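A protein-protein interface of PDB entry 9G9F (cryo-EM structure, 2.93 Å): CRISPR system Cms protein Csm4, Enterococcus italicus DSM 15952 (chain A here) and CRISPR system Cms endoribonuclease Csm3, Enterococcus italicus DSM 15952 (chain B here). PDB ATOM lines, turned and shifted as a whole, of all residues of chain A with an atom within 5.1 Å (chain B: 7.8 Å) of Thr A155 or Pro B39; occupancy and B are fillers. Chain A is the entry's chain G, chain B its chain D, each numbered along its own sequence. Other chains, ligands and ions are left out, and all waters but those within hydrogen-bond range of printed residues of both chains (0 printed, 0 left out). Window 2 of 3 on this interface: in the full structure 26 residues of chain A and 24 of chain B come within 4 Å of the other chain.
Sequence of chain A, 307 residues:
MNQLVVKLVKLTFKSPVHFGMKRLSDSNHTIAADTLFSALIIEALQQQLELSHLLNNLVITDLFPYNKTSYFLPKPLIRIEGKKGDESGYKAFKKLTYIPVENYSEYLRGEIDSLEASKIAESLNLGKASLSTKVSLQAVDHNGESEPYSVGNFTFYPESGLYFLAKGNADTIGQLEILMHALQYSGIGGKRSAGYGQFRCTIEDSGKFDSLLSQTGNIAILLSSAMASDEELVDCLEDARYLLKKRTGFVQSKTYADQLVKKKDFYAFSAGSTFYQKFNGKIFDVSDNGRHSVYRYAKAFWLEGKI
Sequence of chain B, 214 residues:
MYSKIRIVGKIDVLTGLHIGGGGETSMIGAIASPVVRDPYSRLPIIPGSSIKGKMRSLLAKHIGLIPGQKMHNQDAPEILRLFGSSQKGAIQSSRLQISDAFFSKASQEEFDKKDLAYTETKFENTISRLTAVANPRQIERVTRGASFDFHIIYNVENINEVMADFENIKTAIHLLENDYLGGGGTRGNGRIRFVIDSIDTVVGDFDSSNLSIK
N of Asp B38 is in hydrogen-bond range of O of Leu B43 (2.9 Å).
The side-chain carboxylate (OD2) of Asp B38 is in hydrogen-bond range of the side-chain hydroxyl (OG) of Ser B41, 3.2 Å away.
The backbone NH (N) of Tyr A157 is in hydrogen-bond range of the backbone carbonyl oxygen (O) of Leu A126 (2.9 Å).
O of Lys A128 sits at hydrogen-bond distance from N of Thr A155, 2.9 Å away.
Phe B102 touches Pro A16.
Lys A128 touches Pro B39 (CD to O, 3.9 Å).
Thr A155 touches Asp B38 (CG2 to OD1, 3.5 Å).
OG1 of Thr A155 touches CD of Pro B39, at 3.1 Å.
CE1 of Tyr A157 touches CB of Tyr B40, 3.7 Å away.
Of the printed residues of chain B, Pro A16 touches Phe B102.
Of the printed residues of chain B, Lys A128 touches Pro B39.
Asn A153 touches none of the printed residues of chain B.
Of the printed residues of chain B, Thr A155 touches Asp B38 and Pro B39.
Printed residues of chain B within 4 Å of Tyr A157: Tyr B40 (3.7 Å).
Of the printed residues of chain A, Tyr B40 touches Tyr A157 (3.7 Å).
Of the printed residues of chain A, Phe B102 touches Pro A16 (3.9 Å).
The nearest residue of chain B that does not touch Thr A155 is Tyr B40 (5.1 Å).
The nearest residue of chain A that does not touch Pro B39 is Ser A130 (4.1 Å).
The nearest printed residue of chain A that does not touch Phe B102 is Thr A155 (6.4 Å).
Hydrophobic or aromatic side chains of chain A that line the printed part of chain B: Pro A16 and Tyr A157.
Along chain A the printed residues that touch a printed residue of chain B span positions 16 to 157.
Of the 10 printed residues of chain B, 4 touch a printed residue of chain A.
Printed residues of chain B that touch a printed residue of chain A: Asp B38, Pro B39, Tyr B40 and Phe B102.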
ATOM      1  N   PRO A  16      -7.683  -5.886  -7.473  1.00  0.00           N
ATOM      2  CA  PRO A  16      -7.663  -4.552  -6.867  1.00  0.00           C
ATOM      3  C   PRO A  16      -6.472  -4.391  -5.936  1.00  0.00           C
ATOM      4  O   PRO A  16      -6.039  -5.342  -5.288  1.00  0.00           O
ATOM      5  CB  PRO A  16      -8.988  -4.489  -6.102  1.00  0.00           C
ATOM      6  CG  PRO A  16      -9.405  -5.902  -5.936  1.00  0.00           C
ATOM      7  CD  PRO A  16      -8.926  -6.606  -7.155  1.00  0.00           C
ATOM      8  N   LEU A 126      -8.898   6.193 -14.902  1.00  0.00           N
ATOM      9  CA  LEU A 126      -7.951   5.246 -14.328  1.00  0.00           C
ATOM     10  C   LEU A 126      -8.667   4.054 -13.711  1.00  0.00           C
ATOM     11  O   LEU A 126      -8.301   2.901 -13.959  1.00  0.00           O
ATOM     12  CB  LEU A 126      -7.081   5.945 -13.290  1.00  0.00           C
ATOM     13  CG  LEU A 126      -5.992   5.077 -12.670  1.00  0.00           C
ATOM     14  CD1 LEU A 126      -5.077   4.545 -13.750  1.00  0.00           C
ATOM     15  CD2 LEU A 126      -5.212   5.857 -11.637  1.00  0.00           C
ATOM     16  N   GLY A 127      -9.699   4.307 -12.917  1.00  0.00           N
ATOM     17  CA  GLY A 127     -10.412   3.221 -12.281  1.00  0.00           C
ATOM     18  C   GLY A 127     -11.365   3.741 -11.228  1.00  0.00           C
ATOM     19  O   GLY A 127     -11.622   4.941 -11.133  1.00  0.00           O
ATOM     20  N   LYS A 128     -11.880   2.806 -10.436  1.00  0.00           N
ATOM     21  CA  LYS A 128     -12.862   3.099  -9.403  1.00  0.00           C
ATOM     22  C   LYS A 128     -12.333   2.636  -8.054  1.00  0.00           C
ATOM     23  O   LYS A 128     -11.838   1.512  -7.930  1.00  0.00           O
ATOM     24  CB  LYS A 128     -14.196   2.419  -9.711  1.00  0.00           C
ATOM     25  CG  LYS A 128     -15.310   2.785  -8.755  1.00  0.00           C
ATOM     26  CD  LYS A 128     -16.652   2.315  -9.277  1.00  0.00           C
ATOM     27  CE  LYS A 128     -17.777   2.708  -8.337  1.00  0.00           C
ATOM     28  NZ  LYS A 128     -17.613   2.095  -6.991  1.00  0.00           N
ATOM     29  N   ALA A 129     -12.446   3.497  -7.048  1.00  0.00           N
ATOM     30  CA  ALA A 129     -12.006   3.188  -5.696  1.00  0.00           C
ATOM     31  C   ALA A 129     -13.194   2.732  -4.861  1.00  0.00           C
ATOM     32  O   ALA A 129     -14.238   3.390  -4.850  1.00  0.00           O
ATOM     33  CB  ALA A 129     -11.341   4.401  -5.047  1.00  0.00           C
ATOM     34  N   SER A 130     -13.029   1.613  -4.163  1.00  0.00           N
ATOM     35  CA  SER A 130     -14.067   1.056  -3.312  1.00  0.00           C
ATOM     36  C   SER A 130     -13.463   0.688  -1.963  1.00  0.00           C
ATOM     37  O   SER A 130     -12.245   0.705  -1.773  1.00  0.00           O
ATOM     38  CB  SER A 130     -14.722  -0.168  -3.965  1.00  0.00           C
ATOM     39  OG  SER A 130     -15.823  -0.634  -3.202  1.00  0.00           O
ATOM     40  N   ASN A 153      -9.635  -0.542  -1.554  1.00  0.00           N
ATOM     41  CA  ASN A 153      -9.008  -1.016  -2.774  1.00  0.00           C
ATOM     42  C   ASN A 153      -9.374  -0.103  -3.936  1.00  0.00           C
ATOM     43  O   ASN A 153     -10.300   0.704  -3.853  1.00  0.00           O
ATOM     44  CB  ASN A 153      -9.409  -2.463  -3.084  1.00  0.00           C
ATOM     45  CG  ASN A 153     -10.865  -2.739  -2.800  1.00  0.00           C
ATOM     46  OD1 ASN A 153     -11.227  -3.133  -1.695  1.00  0.00           O
ATOM     47  ND2 ASN A 153     -11.709  -2.545  -3.802  1.00  0.00           N
ATOM     48  N   PHE A 154      -8.618  -0.231  -5.022  1.00  0.00           N
ATOM     49  CA  PHE A 154      -8.806   0.594  -6.209  1.00  0.00           C
ATOM     50  C   PHE A 154      -8.695  -0.300  -7.434  1.00  0.00           C
ATOM     51  O   PHE A 154      -7.594  -0.734  -7.784  1.00  0.00           O
ATOM     52  CB  PHE A 154      -7.776   1.718  -6.265  1.00  0.00           C
ATOM     53  CG  PHE A 154      -7.953   2.641  -7.428  1.00  0.00           C
ATOM     54  CD1 PHE A 154      -8.948   3.595  -7.424  1.00  0.00           C
ATOM     55  CD2 PHE A 154      -7.119   2.560  -8.524  1.00  0.00           C
ATOM     56  CE1 PHE A 154      -9.112   4.442  -8.487  1.00  0.00           C
ATOM     57  CE2 PHE A 154      -7.280   3.408  -9.592  1.00  0.00           C
ATOM     58  CZ  PHE A 154      -8.277   4.350  -9.573  1.00  0.00           C
ATOM     59  N   THR A 155      -9.821  -0.569  -8.086  1.00  0.00           N
ATOM     60  CA  THR A 155      -9.845  -1.442  -9.251  1.00  0.00           C
ATOM     61  C   THR A 155      -9.715  -0.608 -10.518  1.00  0.00           C
ATOM     62  O   THR A 155     -10.570   0.237 -10.803  1.00  0.00           O
ATOM     63  CB  THR A 155     -11.129  -2.261  -9.281  1.00  0.00           C
ATOM     64  OG1 THR A 155     -11.284  -2.935  -8.029  1.00  0.00           O
ATOM     65  CG2 THR A 155     -11.068  -3.288 -10.395  1.00  0.00           C
ATOM     66  N   PHE A 156      -8.651  -0.851 -11.274  1.00  0.00           N
ATOM     67  CA  PHE A 156      -8.391  -0.101 -12.493  1.00  0.00           C
ATOM     68  C   PHE A 156      -9.289  -0.581 -13.625  1.00  0.00           C
ATOM     69  O   PHE A 156      -9.626  -1.764 -13.713  1.00  0.00           O
ATOM     70  CB  PHE A 156      -6.923  -0.236 -12.891  1.00  0.00           C
ATOM     71  CG  PHE A 156      -5.973   0.328 -11.878  1.00  0.00           C
ATOM     72  CD1 PHE A 156      -5.614  -0.398 -10.760  1.00  0.00           C
ATOM     73  CD2 PHE A 156      -5.438   1.587 -12.044  1.00  0.00           C
ATOM     74  CE1 PHE A 156      -4.744   0.123  -9.828  1.00  0.00           C
ATOM     75  CE2 PHE A 156      -4.568   2.110 -11.115  1.00  0.00           C
ATOM     76  CZ  PHE A 156      -4.221   1.376 -10.007  1.00  0.00           C
ATOM     77  N   TYR A 157      -9.673   0.348 -14.494  1.00  0.00           N
ATOM     78  CA  TYR A 157     -10.502   0.007 -15.636  1.00  0.00           C
ATOM     79  C   TYR A 157      -9.715  -0.878 -16.603  1.00  0.00           C
ATOM     80  O   TYR A 157      -8.484  -0.828 -16.632  1.00  0.00           O
ATOM     81  CB  TYR A 157     -10.988   1.274 -16.332  1.00  0.00           C
ATOM     82  CG  TYR A 157     -12.140   1.934 -15.613  1.00  0.00           C
ATOM     83  CD1 TYR A 157     -12.948   1.209 -14.753  1.00  0.00           C
ATOM     84  CD2 TYR A 157     -12.418   3.280 -15.788  1.00  0.00           C
ATOM     85  CE1 TYR A 157     -14.001   1.805 -14.090  1.00  0.00           C
ATOM     86  CE2 TYR A 157     -13.469   3.885 -15.128  1.00  0.00           C
ATOM     87  CZ  TYR A 157     -14.256   3.143 -14.283  1.00  0.00           C
ATOM     88  OH  TYR A 157     -15.304   3.741 -13.625  1.00  0.00           O
ATOM     89  N   VAL B  36     -19.818  -9.465  -2.499  1.00  0.00           N
ATOM     90  CA  VAL B  36     -18.860  -8.518  -3.046  1.00  0.00           C
ATOM     91  C   VAL B  36     -18.876  -8.615  -4.566  1.00  0.00           C
ATOM     92  O   VAL B  36     -19.114  -9.682  -5.143  1.00  0.00           O
ATOM     93  CB  VAL B  36     -17.443  -8.757  -2.495  1.00  0.00           C
ATOM     94  CG1 VAL B  36     -17.383  -8.430  -1.019  1.00  0.00           C
ATOM     95  CG2 VAL B  36     -17.009 -10.172  -2.753  1.00  0.00           C
ATOM     96  N   ARG B  37     -18.641  -7.484  -5.220  1.00  0.00           N
ATOM     97  CA  ARG B  37     -18.574  -7.421  -6.668  1.00  0.00           C
ATOM     98  C   ARG B  37     -17.291  -6.715  -7.072  1.00  0.00           C
ATOM     99  O   ARG B  37     -16.721  -5.945  -6.297  1.00  0.00           O
ATOM    100  CB  ARG B  37     -19.762  -6.665  -7.270  1.00  0.00           C
ATOM    101  CG  ARG B  37     -21.071  -6.809  -6.527  1.00  0.00           C
ATOM    102  CD  ARG B  37     -21.772  -8.109  -6.845  1.00  0.00           C
ATOM    103  NE  ARG B  37     -23.218  -7.928  -6.852  1.00  0.00           N
ATOM    104  CZ  ARG B  37     -23.993  -8.147  -7.904  1.00  0.00           C
ATOM    105  NH1 ARG B  37     -23.505  -8.636  -9.031  1.00  0.00           N
ATOM    106  NH2 ARG B  37     -25.289  -7.869  -7.823  1.00  0.00           N
ATOM    107  N   ASP B  38     -16.843  -6.986  -8.284  1.00  0.00           N
ATOM    108  CA  ASP B  38     -15.809  -6.159  -8.880  1.00  0.00           C
ATOM    109  C   ASP B  38     -16.375  -4.758  -9.083  1.00  0.00           C
ATOM    110  O   ASP B  38     -17.488  -4.620  -9.599  1.00  0.00           O
ATOM    111  CB  ASP B  38     -15.351  -6.756 -10.204  1.00  0.00           C
ATOM    112  CG  ASP B  38     -14.068  -6.140 -10.706  1.00  0.00           C
ATOM    113  OD1 ASP B  38     -13.097  -6.073  -9.926  1.00  0.00           O
ATOM    114  OD2 ASP B  38     -14.024  -5.734 -11.885  1.00  0.00           O
ATOM    115  N   PRO B  39     -15.667  -3.705  -8.667  1.00  0.00           N
ATOM    116  CA  PRO B  39     -16.282  -2.365  -8.685  1.00  0.00           C
ATOM    117  C   PRO B  39     -16.747  -1.921 -10.060  1.00  0.00           C
ATOM    118  O   PRO B  39     -17.788  -1.263 -10.174  1.00  0.00           O
ATOM    119  CB  PRO B  39     -15.162  -1.466  -8.147  1.00  0.00           C
ATOM    120  CG  PRO B  39     -14.302  -2.374  -7.346  1.00  0.00           C
ATOM    121  CD  PRO B  39     -14.327  -3.689  -8.063  1.00  0.00           C
ATOM    122  N   TYR B  40     -16.012  -2.273 -11.111  1.00  0.00           N
ATOM    123  CA  TYR B  40     -16.382  -1.868 -12.461  1.00  0.00           C
ATOM    124  C   TYR B  40     -17.256  -2.908 -13.155  1.00  0.00           C
ATOM    125  O   TYR B  40     -18.332  -2.577 -13.661  1.00  0.00           O
ATOM    126  CB  TYR B  40     -15.120  -1.594 -13.283  1.00  0.00           C
ATOM    127  CG  TYR B  40     -15.290  -1.831 -14.765  1.00  0.00           C
ATOM    128  CD1 TYR B  40     -16.051  -0.971 -15.545  1.00  0.00           C
ATOM    129  CD2 TYR B  40     -14.680  -2.913 -15.385  1.00  0.00           C
ATOM    130  CE1 TYR B  40     -16.207  -1.187 -16.898  1.00  0.00           C
ATOM    131  CE2 TYR B  40     -14.831  -3.137 -16.737  1.00  0.00           C
ATOM    132  CZ  TYR B  40     -15.593  -2.271 -17.489  1.00  0.00           C
ATOM    133  OH  TYR B  40     -15.743  -2.492 -18.839  1.00  0.00           O
ATOM    134  N   SER B  41     -16.813  -4.166 -13.183  1.00  0.00           N
ATOM    135  CA  SER B  41     -17.525  -5.202 -13.918  1.00  0.00           C
ATOM    136  C   SER B  41     -18.810  -5.641 -13.237  1.00  0.00           C
ATOM    137  O   SER B  41     -19.669  -6.233 -13.899  1.00  0.00           O
ATOM    138  CB  SER B  41     -16.620  -6.417 -14.119  1.00  0.00           C
ATOM    139  OG  SER B  41     -15.402  -6.048 -14.739  1.00  0.00           O
ATOM    140  N   ARG B  42     -18.952  -5.383 -11.937  1.00  0.00           N
ATOM    141  CA  ARG B  42     -20.120  -5.772 -11.149  1.00  0.00           C
ATOM    142  C   ARG B  42     -20.284  -7.286 -11.073  1.00  0.00           C
ATOM    143  O   ARG B  42     -21.302  -7.775 -10.577  1.00  0.00           O
ATOM    144  CB  ARG B  42     -21.391  -5.132 -11.712  1.00  0.00           C
ATOM    145  CG  ARG B  42     -21.559  -3.665 -11.366  1.00  0.00           C
ATOM    146  CD  ARG B  42     -22.359  -3.474 -10.089  1.00  0.00           C
ATOM    147  NE  ARG B  42     -21.505  -3.165  -8.949  1.00  0.00           N
ATOM    148  CZ  ARG B  42     -21.950  -2.933  -7.722  1.00  0.00           C
ATOM    149  NH1 ARG B  42     -23.242  -2.963  -7.438  1.00  0.00           N
ATOM    150  NH2 ARG B  42     -21.078  -2.660  -6.756  1.00  0.00           N
ATOM    151  N   LEU B  43     -19.298  -8.036 -11.552  1.00  0.00           N
ATOM    152  CA  LEU B  43     -19.345  -9.485 -11.430  1.00  0.00           C
ATOM    153  C   LEU B  43     -19.006  -9.896 -10.001  1.00  0.00           C
ATOM    154  O   LEU B  43     -18.077  -9.347  -9.403  1.00  0.00           O
ATOM    155  CB  LEU B  43     -18.362 -10.139 -12.395  1.00  0.00           C
ATOM    156  CG  LEU B  43     -18.642  -9.994 -13.885  1.00  0.00           C
ATOM    157  CD1 LEU B  43     -17.463 -10.507 -14.678  1.00  0.00           C
ATOM    158  CD2 LEU B  43     -19.905 -10.742 -14.254  1.00  0.00           C
ATOM    159  N   ILE B  45     -17.276 -11.806  -7.004  1.00  0.00           N
ATOM    160  CA  ILE B  45     -15.934 -12.346  -6.861  1.00  0.00           C
ATOM    161  C   ILE B  45     -15.819 -13.024  -5.504  1.00  0.00           C
ATOM    162  O   ILE B  45     -16.688 -12.900  -4.642  1.00  0.00           O
ATOM    163  CB  ILE B  45     -14.838 -11.271  -7.008  1.00  0.00           C
ATOM    164  CG1 ILE B  45     -14.908 -10.275  -5.855  1.00  0.00           C
ATOM    165  CG2 ILE B  45     -14.964 -10.558  -8.338  1.00  0.00           C
ATOM    166  CD1 ILE B  45     -13.747  -9.321  -5.818  1.00  0.00           C
ATOM    167  N   PHE B 102     -11.993 -14.398  -9.505  1.00  0.00           N
ATOM    168  CA  PHE B 102     -12.922 -13.644 -10.329  1.00  0.00           C
ATOM    169  C   PHE B 102     -13.785 -14.586 -11.157  1.00  0.00           C
ATOM    170  O   PHE B 102     -13.403 -15.725 -11.428  1.00  0.00           O
ATOM    171  CB  PHE B 102     -12.168 -12.683 -11.249  1.00  0.00           C
ATOM    172  CG  PHE B 102     -11.345 -11.670 -10.512  1.00  0.00           C
ATOM    173  CD1 PHE B 102     -11.928 -10.524 -10.002  1.00  0.00           C
ATOM    174  CD2 PHE B 102      -9.989 -11.866 -10.318  1.00  0.00           C
ATOM    175  CE1 PHE B 102     -11.178  -9.594  -9.317  1.00  0.00           C
ATOM    176  CE2 PHE B 102      -9.232 -10.936  -9.634  1.00  0.00           C
ATOM    177  CZ  PHE B 102      -9.828  -9.800  -9.133  1.00  0.00           C
